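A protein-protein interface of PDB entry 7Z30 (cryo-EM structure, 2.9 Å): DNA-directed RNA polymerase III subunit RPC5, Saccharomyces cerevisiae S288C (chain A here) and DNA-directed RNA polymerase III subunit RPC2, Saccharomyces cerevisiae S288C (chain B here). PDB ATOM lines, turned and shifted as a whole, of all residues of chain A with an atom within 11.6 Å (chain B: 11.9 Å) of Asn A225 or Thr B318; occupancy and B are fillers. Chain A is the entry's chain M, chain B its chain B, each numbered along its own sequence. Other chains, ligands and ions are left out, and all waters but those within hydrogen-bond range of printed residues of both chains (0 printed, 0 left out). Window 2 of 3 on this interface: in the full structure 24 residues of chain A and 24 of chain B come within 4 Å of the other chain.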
ATOM      1  N   ASN A 225      18.335 -13.908 -11.300  1.00  0.00           N
ATOM      2  CA  ASN A 225      17.886 -13.005 -10.206  1.00  0.00           C
ATOM      3  C   ASN A 225      16.582 -13.547  -9.611  1.00  0.00           C
ATOM      4  O   ASN A 225      15.627 -12.757  -9.472  1.00  0.00           O
ATOM      5  CB  ASN A 225      17.726 -11.562 -10.691  1.00  0.00           C
ATOM      6  CG  ASN A 225      19.017 -10.967 -11.214  1.00  0.00           C
ATOM      7  OD1 ASN A 225      19.953 -11.693 -11.539  1.00  0.00           O
ATOM      8  ND2 ASN A 225      19.076  -9.648 -11.293  1.00  0.00           N
ATOM      9  N   ARG A 226      16.553 -14.837  -9.266  1.00  0.00           N
ATOM     10  CA  ARG A 226      15.321 -15.462  -8.714  1.00  0.00           C
ATOM     11  C   ARG A 226      14.906 -14.722  -7.439  1.00  0.00           C
ATOM     12  O   ARG A 226      13.695 -14.476  -7.274  1.00  0.00           O
ATOM     13  CB  ARG A 226      15.562 -16.946  -8.423  1.00  0.00           C
ATOM     14  CG  ARG A 226      14.362 -17.836  -8.704  1.00  0.00           C
ATOM     15  CD  ARG A 226      14.520 -18.629  -9.987  1.00  0.00           C
ATOM     16  NE  ARG A 226      14.491 -17.786 -11.173  1.00  0.00           N
ATOM     17  CZ  ARG A 226      15.546 -17.527 -11.938  1.00  0.00           C
ATOM     18  NH1 ARG A 226      15.877 -16.278 -12.208  1.00  0.00           N
ATOM     19  NH2 ARG A 226      16.267 -18.521 -12.427  1.00  0.00           N
ATOM     20  N   LEU A 227      15.874 -14.398  -6.575  1.00  0.00           N
ATOM     21  CA  LEU A 227      15.580 -13.659  -5.317  1.00  0.00           C
ATOM     22  C   LEU A 227      14.469 -14.381  -4.549  1.00  0.00           C
ATOM     23  O   LEU A 227      13.544 -13.697  -4.078  1.00  0.00           O
ATOM     24  CB  LEU A 227      15.171 -12.224  -5.664  1.00  0.00           C
ATOM     25  CG  LEU A 227      16.019 -11.140  -5.003  1.00  0.00           C
ATOM     26  CD1 LEU A 227      15.155 -10.230  -4.144  1.00  0.00           C
ATOM     27  CD2 LEU A 227      17.122 -11.772  -4.170  1.00  0.00           C
ATOM     28  N   THR A 228      14.571 -15.708  -4.427  1.00  0.00           N
ATOM     29  CA  THR A 228      13.557 -16.500  -3.681  1.00  0.00           C
ATOM     30  C   THR A 228      13.884 -16.472  -2.183  1.00  0.00           C
ATOM     31  O   THR A 228      14.868 -15.805  -1.809  1.00  0.00           O
ATOM     32  CB  THR A 228      13.473 -17.932  -4.227  1.00  0.00           C
ATOM     33  OG1 THR A 228      12.540 -18.663  -3.430  1.00  0.00           O
ATOM     34  CG2 THR A 228      14.812 -18.638  -4.228  1.00  0.00           C
ATOM     35  N   GLY A 229      13.087 -17.165  -1.365  1.00  0.00           N
ATOM     36  CA  GLY A 229      13.303 -17.174   0.095  1.00  0.00           C
ATOM     37  C   GLY A 229      12.643 -15.980   0.762  1.00  0.00           C
ATOM     38  O   GLY A 229      11.689 -15.435   0.176  1.00  0.00           O
ATOM     39  N   SER A 230      13.121 -15.592   1.947  1.00  0.00           N
ATOM     40  CA  SER A 230      12.578 -14.381   2.616  1.00  0.00           C
ATOM     41  C   SER A 230      12.676 -13.192   1.655  1.00  0.00           C
ATOM     42  O   SER A 230      11.831 -12.282   1.757  1.00  0.00           O
ATOM     43  CB  SER A 230      13.287 -14.101   3.913  1.00  0.00           C
ATOM     44  OG  SER A 230      12.406 -13.489   4.844  1.00  0.00           O
ATOM     45  N   LEU A 231      13.666 -13.203   0.755  1.00  0.00           N
ATOM     46  CA  LEU A 231      13.750 -12.134  -0.232  1.00  0.00           C
ATOM     47  C   LEU A 231      12.505 -12.122  -1.107  1.00  0.00           C
ATOM     48  O   LEU A 231      11.927 -11.063  -1.379  1.00  0.00           O
ATOM     49  CB  LEU A 231      15.000 -12.317  -1.091  1.00  0.00           C
ATOM     50  CG  LEU A 231      16.341 -11.752  -0.622  1.00  0.00           C
ATOM     51  CD1 LEU A 231      16.245 -10.244  -0.465  1.00  0.00           C
ATOM     52  CD2 LEU A 231      16.814 -12.417   0.662  1.00  0.00           C
ATOM     53  N   LEU A 232      12.072 -13.306  -1.549  1.00  0.00           N
ATOM     54  CA  LEU A 232      10.872 -13.402  -2.367  1.00  0.00           C
ATOM     55  C   LEU A 232       9.631 -12.979  -1.594  1.00  0.00           C
ATOM     56  O   LEU A 232       8.682 -12.466  -2.190  1.00  0.00           O
ATOM     57  CB  LEU A 232      10.709 -14.825  -2.899  1.00  0.00           C
ATOM     58  CG  LEU A 232       9.604 -15.027  -3.938  1.00  0.00           C
ATOM     59  CD1 LEU A 232       9.720 -13.988  -5.040  1.00  0.00           C
ATOM     60  CD2 LEU A 232       9.652 -16.432  -4.516  1.00  0.00           C
ATOM     61  N   ALA A 233       9.619 -13.169  -0.274  1.00  0.00           N
ATOM     62  CA  ALA A 233       8.455 -12.776   0.514  1.00  0.00           C
ATOM     63  C   ALA A 233       8.241 -11.267   0.466  1.00  0.00           C
ATOM     64  O   ALA A 233       7.140 -10.790   0.162  1.00  0.00           O
ATOM     65  CB  ALA A 233       8.613 -13.256   1.957  1.00  0.00           C
ATOM     66  N   LYS A 235       9.674  -9.245  -1.701  1.00  0.00           N
ATOM     67  CA  LYS A 235       9.486  -8.924  -3.112  1.00  0.00           C
ATOM     68  C   LYS A 235       8.016  -9.034  -3.499  1.00  0.00           C
ATOM     69  O   LYS A 235       7.462  -8.138  -4.144  1.00  0.00           O
ATOM     70  CB  LYS A 235      10.343  -9.852  -3.974  1.00  0.00           C
ATOM     71  CG  LYS A 235      10.822  -9.244  -5.282  1.00  0.00           C
ATOM     72  CD  LYS A 235      11.934  -8.233  -5.059  1.00  0.00           C
ATOM     73  CE  LYS A 235      12.688  -7.956  -6.350  1.00  0.00           C
ATOM     74  NZ  LYS A 235      13.944  -7.191  -6.117  1.00  0.00           N
ATOM     75  N   VAL A 236       7.364 -10.124  -3.096  1.00  0.00           N
ATOM     76  CA  VAL A 236       5.935 -10.280  -3.336  1.00  0.00           C
ATOM     77  C   VAL A 236       5.157  -9.184  -2.625  1.00  0.00           C
ATOM     78  O   VAL A 236       4.277  -8.547  -3.214  1.00  0.00           O
ATOM     79  CB  VAL A 236       5.478 -11.685  -2.899  1.00  0.00           C
ATOM     80  CG1 VAL A 236       4.012 -11.678  -2.484  1.00  0.00           C
ATOM     81  CG2 VAL A 236       5.722 -12.692  -4.010  1.00  0.00           C
ATOM     82  N   ASP A 238       5.904  -6.122  -1.715  1.00  0.00           N
ATOM     83  CA  ASP A 238       5.977  -4.790  -2.306  1.00  0.00           C
ATOM     84  C   ASP A 238       5.722  -4.772  -3.812  1.00  0.00           C
ATOM     85  O   ASP A 238       5.616  -3.685  -4.387  1.00  0.00           O
ATOM     86  CB  ASP A 238       7.326  -4.121  -1.979  1.00  0.00           C
ATOM     87  CG  ASP A 238       8.522  -4.828  -2.601  1.00  0.00           C
ATOM     88  OD1 ASP A 238       8.345  -5.782  -3.378  1.00  0.00           O
ATOM     89  OD2 ASP A 238       9.662  -4.412  -2.304  1.00  0.00           O
ATOM     90  N   GLU A 239       5.620  -5.931  -4.467  1.00  0.00           N
ATOM     91  CA  GLU A 239       5.265  -5.956  -5.884  1.00  0.00           C
ATOM     92  C   GLU A 239       3.771  -6.192  -6.095  1.00  0.00           C
ATOM     93  O   GLU A 239       3.080  -5.347  -6.672  1.00  0.00           O
ATOM     94  CB  GLU A 239       6.086  -7.026  -6.613  1.00  0.00           C
ATOM     95  CG  GLU A 239       7.501  -6.593  -6.952  1.00  0.00           C
ATOM     96  CD  GLU A 239       8.154  -7.496  -7.977  1.00  0.00           C
ATOM     97  OE1 GLU A 239       7.489  -7.839  -8.978  1.00  0.00           O
ATOM     98  OE2 GLU A 239       9.333  -7.857  -7.788  1.00  0.00           O
ATOM     99  N   GLY B 306      21.719  -3.596   6.471  1.00  0.00           N
ATOM    100  CA  GLY B 306      22.179  -3.941   5.138  1.00  0.00           C
ATOM    101  C   GLY B 306      23.359  -3.126   4.659  1.00  0.00           C
ATOM    102  O   GLY B 306      24.144  -3.613   3.838  1.00  0.00           O
ATOM    103  N   THR B 311      30.474  -8.462   1.680  1.00  0.00           N
ATOM    104  CA  THR B 311      30.627  -8.847   0.281  1.00  0.00           C
ATOM    105  C   THR B 311      30.095 -10.261   0.095  1.00  0.00           C
ATOM    106  O   THR B 311      29.839 -10.984   1.062  1.00  0.00           O
ATOM    107  CB  THR B 311      32.088  -8.765  -0.175  1.00  0.00           C
ATOM    108  OG1 THR B 311      32.179  -9.112  -1.563  1.00  0.00           O
ATOM    109  CG2 THR B 311      32.958  -9.715   0.640  1.00  0.00           C
ATOM    110  N   MET B 312      29.926 -10.642  -1.170  1.00  0.00           N
ATOM    111  CA  MET B 312      29.524 -11.992  -1.554  1.00  0.00           C
ATOM    112  C   MET B 312      30.309 -12.454  -2.776  1.00  0.00           C
ATOM    113  O   MET B 312      29.778 -13.137  -3.658  1.00  0.00           O
ATOM    114  CB  MET B 312      28.019 -12.062  -1.810  1.00  0.00           C
ATOM    115  CG  MET B 312      27.551 -11.182  -2.954  1.00  0.00           C
ATOM    116  SD  MET B 312      25.909 -10.505  -2.680  1.00  0.00           S
ATOM    117  CE  MET B 312      26.316  -8.771  -2.528  1.00  0.00           C
ATOM    118  N   ARG B 313      31.594 -12.095  -2.831  1.00  0.00           N
ATOM    119  CA  ARG B 313      32.476 -12.425  -3.954  1.00  0.00           C
ATOM    120  C   ARG B 313      31.960 -11.860  -5.276  1.00  0.00           C
ATOM    121  O   ARG B 313      32.166 -12.452  -6.338  1.00  0.00           O
ATOM    122  CB  ARG B 313      32.704 -13.938  -4.064  1.00  0.00           C
ATOM    123  CG  ARG B 313      32.910 -14.634  -2.725  1.00  0.00           C
ATOM    124  CD  ARG B 313      34.363 -14.545  -2.285  1.00  0.00           C
ATOM    125  NE  ARG B 313      34.638 -15.365  -1.110  1.00  0.00           N
ATOM    126  CZ  ARG B 313      35.557 -15.077  -0.197  1.00  0.00           C
ATOM    127  NH1 ARG B 313      36.309 -13.993  -0.292  1.00  0.00           N
ATOM    128  NH2 ARG B 313      35.725 -15.897   0.836  1.00  0.00           N
ATOM    129  N   ARG B 314      31.294 -10.705  -5.208  1.00  0.00           N
ATOM    130  CA  ARG B 314      30.879  -9.938  -6.386  1.00  0.00           C
ATOM    131  C   ARG B 314      30.034 -10.773  -7.349  1.00  0.00           C
ATOM    132  O   ARG B 314      30.255 -10.782  -8.563  1.00  0.00           O
ATOM    133  CB  ARG B 314      32.092  -9.335  -7.097  1.00  0.00           C
ATOM    134  CG  ARG B 314      32.648  -8.101  -6.402  1.00  0.00           C
ATOM    135  CD  ARG B 314      33.842  -7.522  -7.142  1.00  0.00           C
ATOM    136  NE  ARG B 314      33.499  -7.109  -8.498  1.00  0.00           N
ATOM    137  CZ  ARG B 314      34.053  -6.082  -9.128  1.00  0.00           C
ATOM    138  NH1 ARG B 314      34.977  -5.332  -8.550  1.00  0.00           N
ATOM    139  NH2 ARG B 314      33.669  -5.798 -10.370  1.00  0.00           N
ATOM    140  N   GLN B 315      29.055 -11.481  -6.795  1.00  0.00           N
ATOM    141  CA  GLN B 315      28.033 -12.158  -7.579  1.00  0.00           C
ATOM    142  C   GLN B 315      26.670 -11.669  -7.118  1.00  0.00           C
ATOM    143  O   GLN B 315      26.477 -11.389  -5.930  1.00  0.00           O
ATOM    144  CB  GLN B 315      28.128 -13.686  -7.452  1.00  0.00           C
ATOM    145  CG  GLN B 315      29.035 -14.338  -8.486  1.00  0.00           C
ATOM    146  CD  GLN B 315      30.367 -14.779  -7.910  1.00  0.00           C
ATOM    147  OE1 GLN B 315      30.506 -14.958  -6.700  1.00  0.00           O
ATOM    148  NE2 GLN B 315      31.355 -14.959  -8.778  1.00  0.00           N
ATOM    149  N   LYS B 316      25.732 -11.559  -8.061  1.00  0.00           N
ATOM    150  CA  LYS B 316      24.424 -10.953  -7.802  1.00  0.00           C
ATOM    151  C   LYS B 316      24.596  -9.526  -7.276  1.00  0.00           C
ATOM    152  O   LYS B 316      24.095  -9.161  -6.211  1.00  0.00           O
ATOM    153  CB  LYS B 316      23.599 -11.815  -6.837  1.00  0.00           C
ATOM    154  CG  LYS B 316      22.123 -11.441  -6.725  1.00  0.00           C
ATOM    155  CD  LYS B 316      21.451 -11.361  -8.083  1.00  0.00           C
ATOM    156  CE  LYS B 316      20.150 -10.580  -8.001  1.00  0.00           C
ATOM    157  NZ  LYS B 316      19.117 -11.308  -7.213  1.00  0.00           N
ATOM    158  N   LEU B 317      25.344  -8.718  -8.035  1.00  0.00           N
ATOM    159  CA  LEU B 317      25.616  -7.344  -7.622  1.00  0.00           C
ATOM    160  C   LEU B 317      24.342  -6.515  -7.536  1.00  0.00           C
ATOM    161  O   LEU B 317      24.278  -5.554  -6.761  1.00  0.00           O
ATOM    162  CB  LEU B 317      26.606  -6.687  -8.585  1.00  0.00           C
ATOM    163  CG  LEU B 317      28.069  -7.129  -8.504  1.00  0.00           C
ATOM    164  CD1 LEU B 317      28.343  -8.277  -9.460  1.00  0.00           C
ATOM    165  CD2 LEU B 317      28.998  -5.956  -8.789  1.00  0.00           C
ATOM    166  N   THR B 318      23.322  -6.869  -8.311  1.00  0.00           N
ATOM    167  CA  THR B 318      22.046  -6.158  -8.312  1.00  0.00           C
ATOM    168  C   THR B 318      21.251  -6.345  -7.017  1.00  0.00           C
ATOM    169  O   THR B 318      20.106  -5.878  -6.955  1.00  0.00           O
ATOM    170  CB  THR B 318      21.205  -6.601  -9.510  1.00  0.00           C
ATOM    171  OG1 THR B 318      21.279  -8.025  -9.647  1.00  0.00           O
ATOM    172  CG2 THR B 318      21.710  -5.944 -10.788  1.00  0.00           C
ATOM    173  N   ILE B 319      21.808  -7.012  -5.999  1.00  0.00           N
ATOM    174  CA  ILE B 319      21.133  -7.160  -4.715  1.00  0.00           C
ATOM    175  C   ILE B 319      21.560  -6.099  -3.709  1.00  0.00           C
ATOM    176  O   ILE B 319      21.045  -6.079  -2.581  1.00  0.00           O
ATOM    177  CB  ILE B 319      21.375  -8.575  -4.143  1.00  0.00           C
ATOM    178  CG1 ILE B 319      20.225  -8.993  -3.226  1.00  0.00           C
ATOM    179  CG2 ILE B 319      22.707  -8.643  -3.408  1.00  0.00           C
ATOM    180  CD1 ILE B 319      18.867  -8.891  -3.873  1.00  0.00           C
ATOM    181  N   LEU B 320      22.466  -5.196  -4.088  1.00  0.00           N
ATOM    182  CA  LEU B 320      23.003  -4.184  -3.178  1.00  0.00           C
ATOM    183  C   LEU B 320      21.944  -3.111  -2.937  1.00  0.00           C
ATOM    184  O   LEU B 320      21.964  -2.024  -3.518  1.00  0.00           O
ATOM    185  CB  LEU B 320      24.278  -3.576  -3.749  1.00  0.00           C
ATOM    186  CG  LEU B 320      25.625  -4.129  -3.279  1.00  0.00           C
ATOM    187  CD1 LEU B 320      25.861  -5.509  -3.851  1.00  0.00           C
ATOM    188  CD2 LEU B 320      26.750  -3.186  -3.676  1.00  0.00           C
ATOM    189  N   GLN B 321      21.002  -3.427  -2.057  1.00  0.00           N
ATOM    190  CA  GLN B 321      19.929  -2.503  -1.708  1.00  0.00           C
ATOM    191  C   GLN B 321      19.508  -2.786  -0.271  1.00  0.00           C
ATOM    192  O   GLN B 321      20.254  -3.401   0.498  1.00  0.00           O
ATOM    193  CB  GLN B 321      18.761  -2.633  -2.698  1.00  0.00           C
ATOM    194  CG  GLN B 321      18.231  -4.047  -2.842  1.00  0.00           C
ATOM    195  CD  GLN B 321      18.592  -4.664  -4.176  1.00  0.00           C
ATOM    196  OE1 GLN B 321      19.432  -4.139  -4.904  1.00  0.00           O
ATOM    197  NE2 GLN B 321      17.956  -5.782  -4.504  1.00  0.00           N
ATOM    198  N   GLU B 322      18.312  -2.323   0.098  1.00  0.00           N
ATOM    199  CA  GLU B 322      17.734  -2.694   1.384  1.00  0.00           C
ATOM    200  C   GLU B 322      17.521  -4.198   1.498  1.00  0.00           C
ATOM    201  O   GLU B 322      17.551  -4.736   2.607  1.00  0.00           O
ATOM    202  CB  GLU B 322      16.414  -1.946   1.591  1.00  0.00           C
ATOM    203  CG  GLU B 322      15.624  -2.353   2.827  1.00  0.00           C
ATOM    204  CD  GLU B 322      14.494  -3.311   2.511  1.00  0.00           C
ATOM    205  OE1 GLU B 322      13.692  -3.008   1.603  1.00  0.00           O
ATOM    206  OE2 GLU B 322      14.406  -4.365   3.173  1.00  0.00           O
ATOM    207  N   GLY B 323      17.333  -4.891   0.373  1.00  0.00           N
ATOM    208  CA  GLY B 323      17.087  -6.322   0.408  1.00  0.00           C
ATOM    209  C   GLY B 323      18.276  -7.155   0.843  1.00  0.00           C
ATOM    210  O   GLY B 323      18.094  -8.318   1.217  1.00  0.00           O
ATOM    211  N   ILE B 324      19.487  -6.593   0.807  1.00  0.00           N
ATOM    212  CA  ILE B 324      20.656  -7.366   1.219  1.00  0.00           C
ATOM    213  C   ILE B 324      20.584  -7.702   2.704  1.00  0.00           C
ATOM    214  O   ILE B 324      21.102  -8.738   3.144  1.00  0.00           O
ATOM    215  CB  ILE B 324      21.959  -6.622   0.864  1.00  0.00           C
ATOM    216  CG1 ILE B 324      23.145  -7.590   0.891  1.00  0.00           C
ATOM    217  CG2 ILE B 324      22.210  -5.466   1.819  1.00  0.00           C
ATOM    218  CD1 ILE B 324      24.489  -6.919   0.693  1.00  0.00           C
ATOM    219  N   GLU B 325      19.937  -6.849   3.503  1.00  0.00           N
ATOM    220  CA  GLU B 325      19.786  -7.161   4.917  1.00  0.00           C
ATOM    221  C   GLU B 325      18.931  -8.400   5.121  1.00  0.00           C
ATOM    222  O   GLU B 325      19.047  -9.064   6.152  1.00  0.00           O
ATOM    223  CB  GLU B 325      19.189  -5.972   5.670  1.00  0.00           C
ATOM    224  CG  GLU B 325      17.696  -5.729   5.461  1.00  0.00           C
ATOM    225  CD  GLU B 325      16.810  -6.732   6.178  1.00  0.00           C
ATOM    226  OE1 GLU B 325      17.146  -7.104   7.323  1.00  0.00           O
ATOM    227  OE2 GLU B 325      15.798  -7.165   5.590  1.00  0.00           O
ATOM    228  N   ALA B 326      18.031  -8.698   4.183  1.00  0.00           N
ATOM    229  CA  ALA B 326      17.217  -9.899   4.320  1.00  0.00           C
ATOM    230  C   ALA B 326      18.096 -11.141   4.300  1.00  0.00           C
ATOM    231  O   ALA B 326      17.947 -12.034   5.139  1.00  0.00           O
ATOM    232  CB  ALA B 326      16.160  -9.953   3.218  1.00  0.00           C
ATOM    233  N   ILE B 327      19.049 -11.194   3.367  1.00  0.00           N
ATOM    234  CA  ILE B 327      20.010 -12.290   3.369  1.00  0.00           C
ATOM    235  C   ILE B 327      20.926 -12.198   4.586  1.00  0.00           C
ATOM    236  O   ILE B 327      21.337 -13.226   5.135  1.00  0.00           O
ATOM    237  CB  ILE B 327      20.798 -12.324   2.042  1.00  0.00           C
ATOM    238  CG1 ILE B 327      21.049 -13.769   1.610  1.00  0.00           C
ATOM    239  CG2 ILE B 327      22.118 -11.572   2.142  1.00  0.00           C
ATOM    240  CD1 ILE B 327      19.789 -14.555   1.337  1.00  0.00           C
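Of the printed residues of chain B, Asn A225 touches Lys B316 and Thr B318. No residue of chain B comes within 4 Å of Arg A226. Leu A227 touches just these residues of chain B: Lys B316 and Ile B319. Printed residues of chain B within 4 Å of Leu A231: Gly B323 (3.2 Å), Ala B326 (3.6 Å) and Ile B327 (3.7 Å). Gly B306 touches none of the printed residues of chain A. Lys B316 touches two residues of chain A. Of chain A, only Asn A225 comes within 4 Å of Thr B318. Ile B319 touches just one residue of chain A: Leu A227 (3.4 Å). Of the printed residues of chain A, Ala B326 touches Leu A231 (3.6 Å). The nearest residue of chain B that does not touch Asn A225 is Ile B319 (6.5 Å). The nearest printed residue of chain A that does not touch Ala B326 is Ser A230 (5.0 Å).
Among the printed residues, merely in contact across the chains: Asn A225 with Lys B316 (3.4 Å), Leu A227 with Lys B316 (3.7 Å), Leu A227 with Ile B319 (3.4 Å), Leu A231 with Gly B323 (3.2 Å), Leu A231 with Ala B326 (3.6 Å) and Leu A231 with Ile B327 (3.7 Å).
Printed residues of chain B that touch a printed residue of chain A: Lys B316, Thr B318, Ile B319, Gly B323, Ala B326 and Ile B327.
The backbone carbonyl oxygen (O) of Leu A227 lies within hydrogen-bond range of the backbone NH (N) of Leu A232 (3.0 Å). The backbone carbonyl oxygen of Thr B318 sits close to the side-chain amide oxygen of Gln B321 (2.8 Å). The backbone carbonyl oxygen (O) of Ile B319 lies close to the side-chain amide oxygen (OE1) of Gln B321 (3.4 Å).
ND2 of Asn A225 is in hydrogen-bond range of OG1 of Thr B318.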
